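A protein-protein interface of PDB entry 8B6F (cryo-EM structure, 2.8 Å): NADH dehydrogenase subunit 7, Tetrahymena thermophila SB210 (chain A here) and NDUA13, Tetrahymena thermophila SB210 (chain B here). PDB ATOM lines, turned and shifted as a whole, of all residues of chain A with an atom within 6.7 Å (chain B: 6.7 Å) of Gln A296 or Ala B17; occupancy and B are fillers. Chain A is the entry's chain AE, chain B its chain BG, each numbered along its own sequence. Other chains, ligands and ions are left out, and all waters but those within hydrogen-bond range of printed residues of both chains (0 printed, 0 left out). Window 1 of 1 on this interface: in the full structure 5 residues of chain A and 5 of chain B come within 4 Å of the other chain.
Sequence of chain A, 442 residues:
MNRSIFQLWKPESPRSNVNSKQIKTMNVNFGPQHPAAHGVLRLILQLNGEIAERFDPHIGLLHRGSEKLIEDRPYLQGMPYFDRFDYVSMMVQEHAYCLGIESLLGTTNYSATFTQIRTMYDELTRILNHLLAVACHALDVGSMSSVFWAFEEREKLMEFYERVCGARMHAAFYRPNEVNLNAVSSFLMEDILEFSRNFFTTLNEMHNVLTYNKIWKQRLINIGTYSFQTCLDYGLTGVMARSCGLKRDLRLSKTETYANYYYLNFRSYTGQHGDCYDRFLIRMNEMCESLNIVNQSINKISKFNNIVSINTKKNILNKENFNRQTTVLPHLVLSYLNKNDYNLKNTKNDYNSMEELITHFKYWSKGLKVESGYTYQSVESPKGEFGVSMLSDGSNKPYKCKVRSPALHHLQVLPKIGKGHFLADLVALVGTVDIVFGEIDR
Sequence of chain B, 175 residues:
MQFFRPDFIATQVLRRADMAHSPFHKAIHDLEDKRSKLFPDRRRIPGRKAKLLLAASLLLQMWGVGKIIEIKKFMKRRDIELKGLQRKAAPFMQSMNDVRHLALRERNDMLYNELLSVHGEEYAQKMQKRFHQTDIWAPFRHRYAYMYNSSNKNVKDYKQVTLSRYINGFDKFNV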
ATOM      1  N   GLN A 116      37.479   5.821  24.017  1.00  0.00           N
ATOM      2  CA  GLN A 116      37.122   4.940  22.910  1.00  0.00           C
ATOM      3  C   GLN A 116      38.337   4.347  22.209  1.00  0.00           C
ATOM      4  O   GLN A 116      38.181   3.687  21.178  1.00  0.00           O
ATOM      5  CB  GLN A 116      36.258   5.661  21.866  1.00  0.00           C
ATOM      6  CG  GLN A 116      35.028   6.360  22.424  1.00  0.00           C
ATOM      7  CD  GLN A 116      33.950   5.390  22.858  1.00  0.00           C
ATOM      8  OE1 GLN A 116      34.018   4.199  22.567  1.00  0.00           O
ATOM      9  NE2 GLN A 116      32.946   5.899  23.561  1.00  0.00           N
ATOM     10  N   TYR A 263      27.672  -1.787  23.327  1.00  0.00           N
ATOM     11  CA  TYR A 263      26.809  -0.627  23.152  1.00  0.00           C
ATOM     12  C   TYR A 263      27.028   0.045  21.800  1.00  0.00           C
ATOM     13  O   TYR A 263      26.806   1.248  21.651  1.00  0.00           O
ATOM     14  CB  TYR A 263      27.028   0.358  24.296  1.00  0.00           C
ATOM     15  CG  TYR A 263      26.629  -0.231  25.625  1.00  0.00           C
ATOM     16  CD1 TYR A 263      25.295  -0.290  26.001  1.00  0.00           C
ATOM     17  CD2 TYR A 263      27.580  -0.756  26.489  1.00  0.00           C
ATOM     18  CE1 TYR A 263      24.918  -0.838  27.204  1.00  0.00           C
ATOM     19  CE2 TYR A 263      27.213  -1.309  27.697  1.00  0.00           C
ATOM     20  CZ  TYR A 263      25.878  -1.349  28.047  1.00  0.00           C
ATOM     21  OH  TYR A 263      25.494  -1.894  29.246  1.00  0.00           O
ATOM     22  N   LEU A 264      27.466  -0.728  20.812  1.00  0.00           N
ATOM     23  CA  LEU A 264      27.556  -0.288  19.429  1.00  0.00           C
ATOM     24  C   LEU A 264      26.738  -1.235  18.566  1.00  0.00           C
ATOM     25  O   LEU A 264      26.727  -2.446  18.802  1.00  0.00           O
ATOM     26  CB  LEU A 264      29.006  -0.260  18.942  1.00  0.00           C
ATOM     27  CG  LEU A 264      29.951   0.688  19.680  1.00  0.00           C
ATOM     28  CD1 LEU A 264      31.352   0.571  19.114  1.00  0.00           C
ATOM     29  CD2 LEU A 264      29.461   2.122  19.607  1.00  0.00           C
ATOM     30  N   ASN A 265      26.049  -0.684  17.573  1.00  0.00           N
ATOM     31  CA  ASN A 265      25.168  -1.465  16.708  1.00  0.00           C
ATOM     32  C   ASN A 265      25.936  -1.832  15.444  1.00  0.00           C
ATOM     33  O   ASN A 265      25.870  -1.139  14.429  1.00  0.00           O
ATOM     34  CB  ASN A 265      23.892  -0.694  16.394  1.00  0.00           C
ATOM     35  CG  ASN A 265      23.057  -0.435  17.629  1.00  0.00           C
ATOM     36  OD1 ASN A 265      23.094   0.653  18.202  1.00  0.00           O
ATOM     37  ND2 ASN A 265      22.306  -1.444  18.056  1.00  0.00           N
ATOM     38  N   PHE A 266      26.671  -2.936  15.514  1.00  0.00           N
ATOM     39  CA  PHE A 266      27.364  -3.506  14.371  1.00  0.00           C
ATOM     40  C   PHE A 266      26.901  -4.942  14.174  1.00  0.00           C
ATOM     41  O   PHE A 266      26.130  -5.486  14.969  1.00  0.00           O
ATOM     42  CB  PHE A 266      28.887  -3.445  14.549  1.00  0.00           C
ATOM     43  CG  PHE A 266      29.401  -4.237  15.716  1.00  0.00           C
ATOM     44  CD1 PHE A 266      29.417  -3.689  16.987  1.00  0.00           C
ATOM     45  CD2 PHE A 266      29.889  -5.520  15.539  1.00  0.00           C
ATOM     46  CE1 PHE A 266      29.896  -4.410  18.059  1.00  0.00           C
ATOM     47  CE2 PHE A 266      30.371  -6.247  16.607  1.00  0.00           C
ATOM     48  CZ  PHE A 266      30.376  -5.691  17.870  1.00  0.00           C
ATOM     49  N   GLU A 289      33.155  -4.170   8.081  1.00  0.00           N
ATOM     50  CA  GLU A 289      32.376  -3.760   9.242  1.00  0.00           C
ATOM     51  C   GLU A 289      33.226  -3.078  10.303  1.00  0.00           C
ATOM     52  O   GLU A 289      32.688  -2.308  11.105  1.00  0.00           O
ATOM     53  CB  GLU A 289      31.667  -4.969   9.852  1.00  0.00           C
ATOM     54  CG  GLU A 289      30.594  -4.610  10.868  1.00  0.00           C
ATOM     55  CD  GLU A 289      29.390  -3.944  10.234  1.00  0.00           C
ATOM     56  OE1 GLU A 289      29.359  -3.830   8.991  1.00  0.00           O
ATOM     57  OE2 GLU A 289      28.474  -3.536  10.975  1.00  0.00           O
ATOM     58  N   LEU A 291      35.180  -0.755   9.648  1.00  0.00           N
ATOM     59  CA  LEU A 291      35.020   0.651   9.294  1.00  0.00           C
ATOM     60  C   LEU A 291      33.788   1.245   9.955  1.00  0.00           C
ATOM     61  O   LEU A 291      33.835   2.359  10.490  1.00  0.00           O
ATOM     62  CB  LEU A 291      34.927   0.811   7.777  1.00  0.00           C
ATOM     63  CG  LEU A 291      36.127   0.378   6.936  1.00  0.00           C
ATOM     64  CD1 LEU A 291      35.855   0.688   5.476  1.00  0.00           C
ATOM     65  CD2 LEU A 291      37.402   1.051   7.407  1.00  0.00           C
ATOM     66  N   ASN A 292      32.667   0.522   9.920  1.00  0.00           N
ATOM     67  CA  ASN A 292      31.458   1.020  10.564  1.00  0.00           C
ATOM     68  C   ASN A 292      31.653   1.151  12.068  1.00  0.00           C
ATOM     69  O   ASN A 292      31.208   2.133  12.674  1.00  0.00           O
ATOM     70  CB  ASN A 292      30.287   0.090  10.246  1.00  0.00           C
ATOM     71  CG  ASN A 292      28.985   0.569  10.844  1.00  0.00           C
ATOM     72  OD1 ASN A 292      28.843   1.739  11.191  1.00  0.00           O
ATOM     73  ND2 ASN A 292      28.022  -0.336  10.963  1.00  0.00           N
ATOM     74  N   ILE A 293      32.315   0.174  12.692  1.00  0.00           N
ATOM     75  CA  ILE A 293      32.553   0.244  14.132  1.00  0.00           C
ATOM     76  C   ILE A 293      33.429   1.442  14.467  1.00  0.00           C
ATOM     77  O   ILE A 293      33.178   2.161  15.442  1.00  0.00           O
ATOM     78  CB  ILE A 293      33.174  -1.071  14.641  1.00  0.00           C
ATOM     79  CG1 ILE A 293      32.213  -2.236  14.403  1.00  0.00           C
ATOM     80  CG2 ILE A 293      33.499  -0.961  16.127  1.00  0.00           C
ATOM     81  CD1 ILE A 293      32.792  -3.596  14.740  1.00  0.00           C
ATOM     82  N   VAL A 294      34.477   1.672  13.674  1.00  0.00           N
ATOM     83  CA  VAL A 294      35.353   2.814  13.914  1.00  0.00           C
ATOM     84  C   VAL A 294      34.583   4.116  13.745  1.00  0.00           C
ATOM     85  O   VAL A 294      34.758   5.063  14.520  1.00  0.00           O
ATOM     86  CB  VAL A 294      36.580   2.752  12.983  1.00  0.00           C
ATOM     87  CG1 VAL A 294      37.364   4.058  13.019  1.00  0.00           C
ATOM     88  CG2 VAL A 294      37.484   1.597  13.375  1.00  0.00           C
ATOM     89  N   ASN A 295      33.725   4.187  12.729  1.00  0.00           N
ATOM     90  CA  ASN A 295      32.930   5.392  12.523  1.00  0.00           C
ATOM     91  C   ASN A 295      32.028   5.658  13.721  1.00  0.00           C
ATOM     92  O   ASN A 295      31.932   6.793  14.200  1.00  0.00           O
ATOM     93  CB  ASN A 295      32.104   5.257  11.245  1.00  0.00           C
ATOM     94  CG  ASN A 295      31.215   6.455  11.002  1.00  0.00           C
ATOM     95  OD1 ASN A 295      31.518   7.564  11.436  1.00  0.00           O
ATOM     96  ND2 ASN A 295      30.106   6.236  10.310  1.00  0.00           N
ATOM     97  N   GLN A 296      31.355   4.620  14.221  1.00  0.00           N
ATOM     98  CA  GLN A 296      30.512   4.790  15.399  1.00  0.00           C
ATOM     99  C   GLN A 296      31.333   5.238  16.599  1.00  0.00           C
ATOM    100  O   GLN A 296      30.937   6.152  17.328  1.00  0.00           O
ATOM    101  CB  GLN A 296      29.782   3.488  15.718  1.00  0.00           C
ATOM    102  CG  GLN A 296      28.742   3.093  14.694  1.00  0.00           C
ATOM    103  CD  GLN A 296      28.146   1.734  14.984  1.00  0.00           C
ATOM    104  OE1 GLN A 296      28.865   0.750  15.136  1.00  0.00           O
ATOM    105  NE2 GLN A 296      26.826   1.676  15.081  1.00  0.00           N
ATOM    106  N   SER A 297      32.491   4.613  16.810  1.00  0.00           N
ATOM    107  CA  SER A 297      33.327   4.964  17.953  1.00  0.00           C
ATOM    108  C   SER A 297      33.770   6.420  17.886  1.00  0.00           C
ATOM    109  O   SER A 297      33.755   7.129  18.898  1.00  0.00           O
ATOM    110  CB  SER A 297      34.539   4.035  18.008  1.00  0.00           C
ATOM    111  OG  SER A 297      35.429   4.418  19.039  1.00  0.00           O
ATOM    112  N   ILE A 298      34.171   6.883  16.702  1.00  0.00           N
ATOM    113  CA  ILE A 298      34.609   8.268  16.559  1.00  0.00           C
ATOM    114  C   ILE A 298      33.433   9.219  16.732  1.00  0.00           C
ATOM    115  O   ILE A 298      33.579  10.309  17.297  1.00  0.00           O
ATOM    116  CB  ILE A 298      35.321   8.468  15.208  1.00  0.00           C
ATOM    117  CG1 ILE A 298      36.624   7.666  15.186  1.00  0.00           C
ATOM    118  CG2 ILE A 298      35.605   9.948  14.963  1.00  0.00           C
ATOM    119  CD1 ILE A 298      37.314   7.629  13.837  1.00  0.00           C
ATOM    120  N   ASN A 299      32.253   8.834  16.243  1.00  0.00           N
ATOM    121  CA  ASN A 299      31.076   9.674  16.433  1.00  0.00           C
ATOM    122  C   ASN A 299      30.700   9.791  17.904  1.00  0.00           C
ATOM    123  O   ASN A 299      30.131  10.806  18.318  1.00  0.00           O
ATOM    124  CB  ASN A 299      29.897   9.119  15.636  1.00  0.00           C
ATOM    125  CG  ASN A 299      30.148   9.127  14.146  1.00  0.00           C
ATOM    126  OD1 ASN A 299      31.018   9.845  13.655  1.00  0.00           O
ATOM    127  ND2 ASN A 299      29.375   8.336  13.412  1.00  0.00           N
ATOM    128  N   LYS A 300      31.000   8.768  18.706  1.00  0.00           N
ATOM    129  CA  LYS A 300      30.683   8.825  20.128  1.00  0.00           C
ATOM    130  C   LYS A 300      31.444   9.931  20.847  1.00  0.00           C
ATOM    131  O   LYS A 300      31.081  10.285  21.973  1.00  0.00           O
ATOM    132  CB  LYS A 300      30.985   7.478  20.789  1.00  0.00           C
ATOM    133  CG  LYS A 300      30.072   6.344  20.345  1.00  0.00           C
ATOM    134  CD  LYS A 300      28.672   6.485  20.903  1.00  0.00           C
ATOM    135  CE  LYS A 300      27.758   5.412  20.340  1.00  0.00           C
ATOM    136  NZ  LYS A 300      26.354   5.594  20.787  1.00  0.00           N
ATOM    137  N   ILE A 301      32.491  10.478  20.232  1.00  0.00           N
ATOM    138  CA  ILE A 301      33.308  11.514  20.857  1.00  0.00           C
ATOM    139  C   ILE A 301      33.305  12.772  19.997  1.00  0.00           C
ATOM    140  O   ILE A 301      34.289  13.517  19.972  1.00  0.00           O
ATOM    141  CB  ILE A 301      34.748  11.017  21.086  1.00  0.00           C
ATOM    142  CG1 ILE A 301      35.322  10.442  19.787  1.00  0.00           C
ATOM    143  CG2 ILE A 301      34.772   9.981  22.194  1.00  0.00           C
ATOM    144  CD1 ILE A 301      36.786  10.071  19.862  1.00  0.00           C
ATOM    145  N   ARG B  16      20.006   3.407  16.066  1.00  0.00           N
ATOM    146  CA  ARG B  16      21.010   2.345  15.784  1.00  0.00           C
ATOM    147  C   ARG B  16      21.453   2.414  14.329  1.00  0.00           C
ATOM    148  O   ARG B  16      20.632   2.344  13.417  1.00  0.00           O
ATOM    149  CB  ARG B  16      20.437   0.968  16.113  1.00  0.00           C
ATOM    150  CG  ARG B  16      19.103   0.672  15.451  1.00  0.00           C
ATOM    151  CD  ARG B  16      18.522  -0.629  15.968  1.00  0.00           C
ATOM    152  NE  ARG B  16      19.387  -1.763  15.669  1.00  0.00           N
ATOM    153  CZ  ARG B  16      19.222  -2.983  16.159  1.00  0.00           C
ATOM    154  NH1 ARG B  16      18.235  -3.265  16.994  1.00  0.00           N
ATOM    155  NH2 ARG B  16      20.065  -3.945  15.801  1.00  0.00           N
ATOM    156  N   ALA B  17      22.764   2.549  14.121  1.00  0.00           N
ATOM    157  CA  ALA B  17      23.280   2.780  12.777  1.00  0.00           C
ATOM    158  C   ALA B  17      22.936   1.638  11.831  1.00  0.00           C
ATOM    159  O   ALA B  17      22.772   1.862  10.627  1.00  0.00           O
ATOM    160  CB  ALA B  17      24.793   2.984  12.824  1.00  0.00           C
ATOM    161  N   ASP B  18      22.824   0.414  12.345  1.00  0.00           N
ATOM    162  CA  ASP B  18      22.581  -0.734  11.481  1.00  0.00           C
ATOM    163  C   ASP B  18      21.172  -0.756  10.901  1.00  0.00           C
ATOM    164  O   ASP B  18      20.899  -1.588  10.030  1.00  0.00           O
ATOM    165  CB  ASP B  18      22.855  -2.034  12.241  1.00  0.00           C
ATOM    166  CG  ASP B  18      22.013  -2.170  13.489  1.00  0.00           C
ATOM    167  OD1 ASP B  18      21.301  -1.206  13.835  1.00  0.00           O
ATOM    168  OD2 ASP B  18      22.062  -3.242  14.127  1.00  0.00           O
ATOM    169  N   MET B  19      20.278   0.119  11.355  1.00  0.00           N
ATOM    170  CA  MET B  19      18.929   0.212  10.819  1.00  0.00           C
ATOM    171  C   MET B  19      18.692   1.599  10.236  1.00  0.00           C
ATOM    172  O   MET B  19      19.357   2.573  10.598  1.00  0.00           O
ATOM    173  CB  MET B  19      17.874  -0.092  11.890  1.00  0.00           C
ATOM    174  CG  MET B  19      17.978  -1.494  12.459  1.00  0.00           C
ATOM    175  SD  MET B  19      16.450  -2.067  13.221  1.00  0.00           S
ATOM    176  CE  MET B  19      15.411  -2.264  11.774  1.00  0.00           C
ATOM    177  N   ALA B  20      17.726   1.672   9.327  1.00  0.00           N
ATOM    178  CA  ALA B  20      17.469   2.895   8.585  1.00  0.00           C
ATOM    179  C   ALA B  20      16.894   3.982   9.489  1.00  0.00           C
ATOM    180  O   ALA B  20      16.313   3.716  10.543  1.00  0.00           O
ATOM    181  CB  ALA B  20      16.499   2.624   7.435  1.00  0.00           C
ATOM    182  N   SER B  22      18.233   6.092  11.377  1.00  0.00           N
ATOM    183  CA  SER B  22      18.820   6.240  12.696  1.00  0.00           C
ATOM    184  C   SER B  22      19.232   7.693  12.927  1.00  0.00           C
ATOM    185  O   SER B  22      19.692   8.362  11.998  1.00  0.00           O
ATOM    186  CB  SER B  22      20.035   5.328  12.846  1.00  0.00           C
ATOM    187  OG  SER B  22      20.585   5.427  14.148  1.00  0.00           O
ATOM    188  N   PHE B  24      21.827   8.652  14.327  1.00  0.00           N
ATOM    189  CA  PHE B  24      23.276   8.756  14.205  1.00  0.00           C
ATOM    190  C   PHE B  24      23.711   9.105  12.787  1.00  0.00           C
ATOM    191  O   PHE B  24      24.746   9.752  12.604  1.00  0.00           O
ATOM    192  CB  PHE B  24      23.926   7.452  14.662  1.00  0.00           C
ATOM    193  CG  PHE B  24      23.644   7.107  16.100  1.00  0.00           C
ATOM    194  CD1 PHE B  24      23.508   8.104  17.053  1.00  0.00           C
ATOM    195  CD2 PHE B  24      23.508   5.788  16.495  1.00  0.00           C
ATOM    196  CE1 PHE B  24      23.246   7.792  18.371  1.00  0.00           C
ATOM    197  CE2 PHE B  24      23.246   5.471  17.815  1.00  0.00           C
ATOM    198  CZ  PHE B  24      23.116   6.474  18.752  1.00  0.00           C
ATOM    199  N   HIS B  25      22.951   8.685  11.778  1.00  0.00           N
ATOM    200  CA  HIS B  25      23.271   9.058  10.407  1.00  0.00           C
ATOM    201  C   HIS B  25      23.207  10.571  10.241  1.00  0.00           C
ATOM    202  O   HIS B  25      22.336  11.237  10.808  1.00  0.00           O
ATOM    203  CB  HIS B  25      22.304   8.385   9.433  1.00  0.00           C
ATOM    204  CG  HIS B  25      22.363   6.890   9.459  1.00  0.00           C
ATOM    205  ND1 HIS B  25      23.455   6.196   9.933  1.00  0.00           N
ATOM    206  CD2 HIS B  25      21.461   5.957   9.074  1.00  0.00           C
ATOM    207  CE1 HIS B  25      23.225   4.898   9.835  1.00  0.00           C
ATOM    208  NE2 HIS B  25      22.021   4.726   9.318  1.00  0.00           N
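Among the printed residues, merely in contact across the chains: Asn A265 with Arg B16 (3.3 Å), Asn A265 with Asp B18 (3.7 Å), Gln A296 with Ala B17 (3.3 Å) and Lys A300 with Phe B24 (3.9 Å).
Printed residues of chain B that touch a printed residue of chain A: Arg B16, Ala B17, Asp B18 and Phe B24.
Hydrophobic or aromatic side chains of chain B that line the printed part of chain A: Ala B17 and Phe B24.
Of chain B, only Ala B17 comes within 4 Å of Gln A296.
Ala B17 touches just one residue of chain A: Gln A296.
Printed residues of chain A within 4 Å of Asp B18: Asn A265 (3.7 Å).
Printed residues of chain A within 4 Å of Phe B24: Lys A300 (3.9 Å).
Printed residues of chain B within 4 Å of Asn A265: Arg B16 and Asp B18.
Of the printed residues of chain A, Arg B16 touches Asn A265.
Of the printed residues of chain B, Lys A300 touches Phe B24 (3.9 Å).
The nearest residue of chain B that does not touch Gln A296 is Asp B18 (5.0 Å).
The nearest printed residue of chain B that does not touch Lys A300 is Arg B16 (8.0 Å).
O of Asn A265 is in hydrogen-bond range of NE2 of Gln A296 (3.0 Å).
The guanidinium group (NH2) of Arg B16 is in salt-bridge range of the side-chain carboxylate (OD2) of Asp B18 (2.7 Å).
N of Arg B16 sits at hydrogen-bond distance from OG of Ser B22, 2.8 Å away.
NE2 of His B25 sits close to O of Ala B17.
The side-chain hydroxyl of Ser B22 sits close to the backbone NH of Phe B24.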
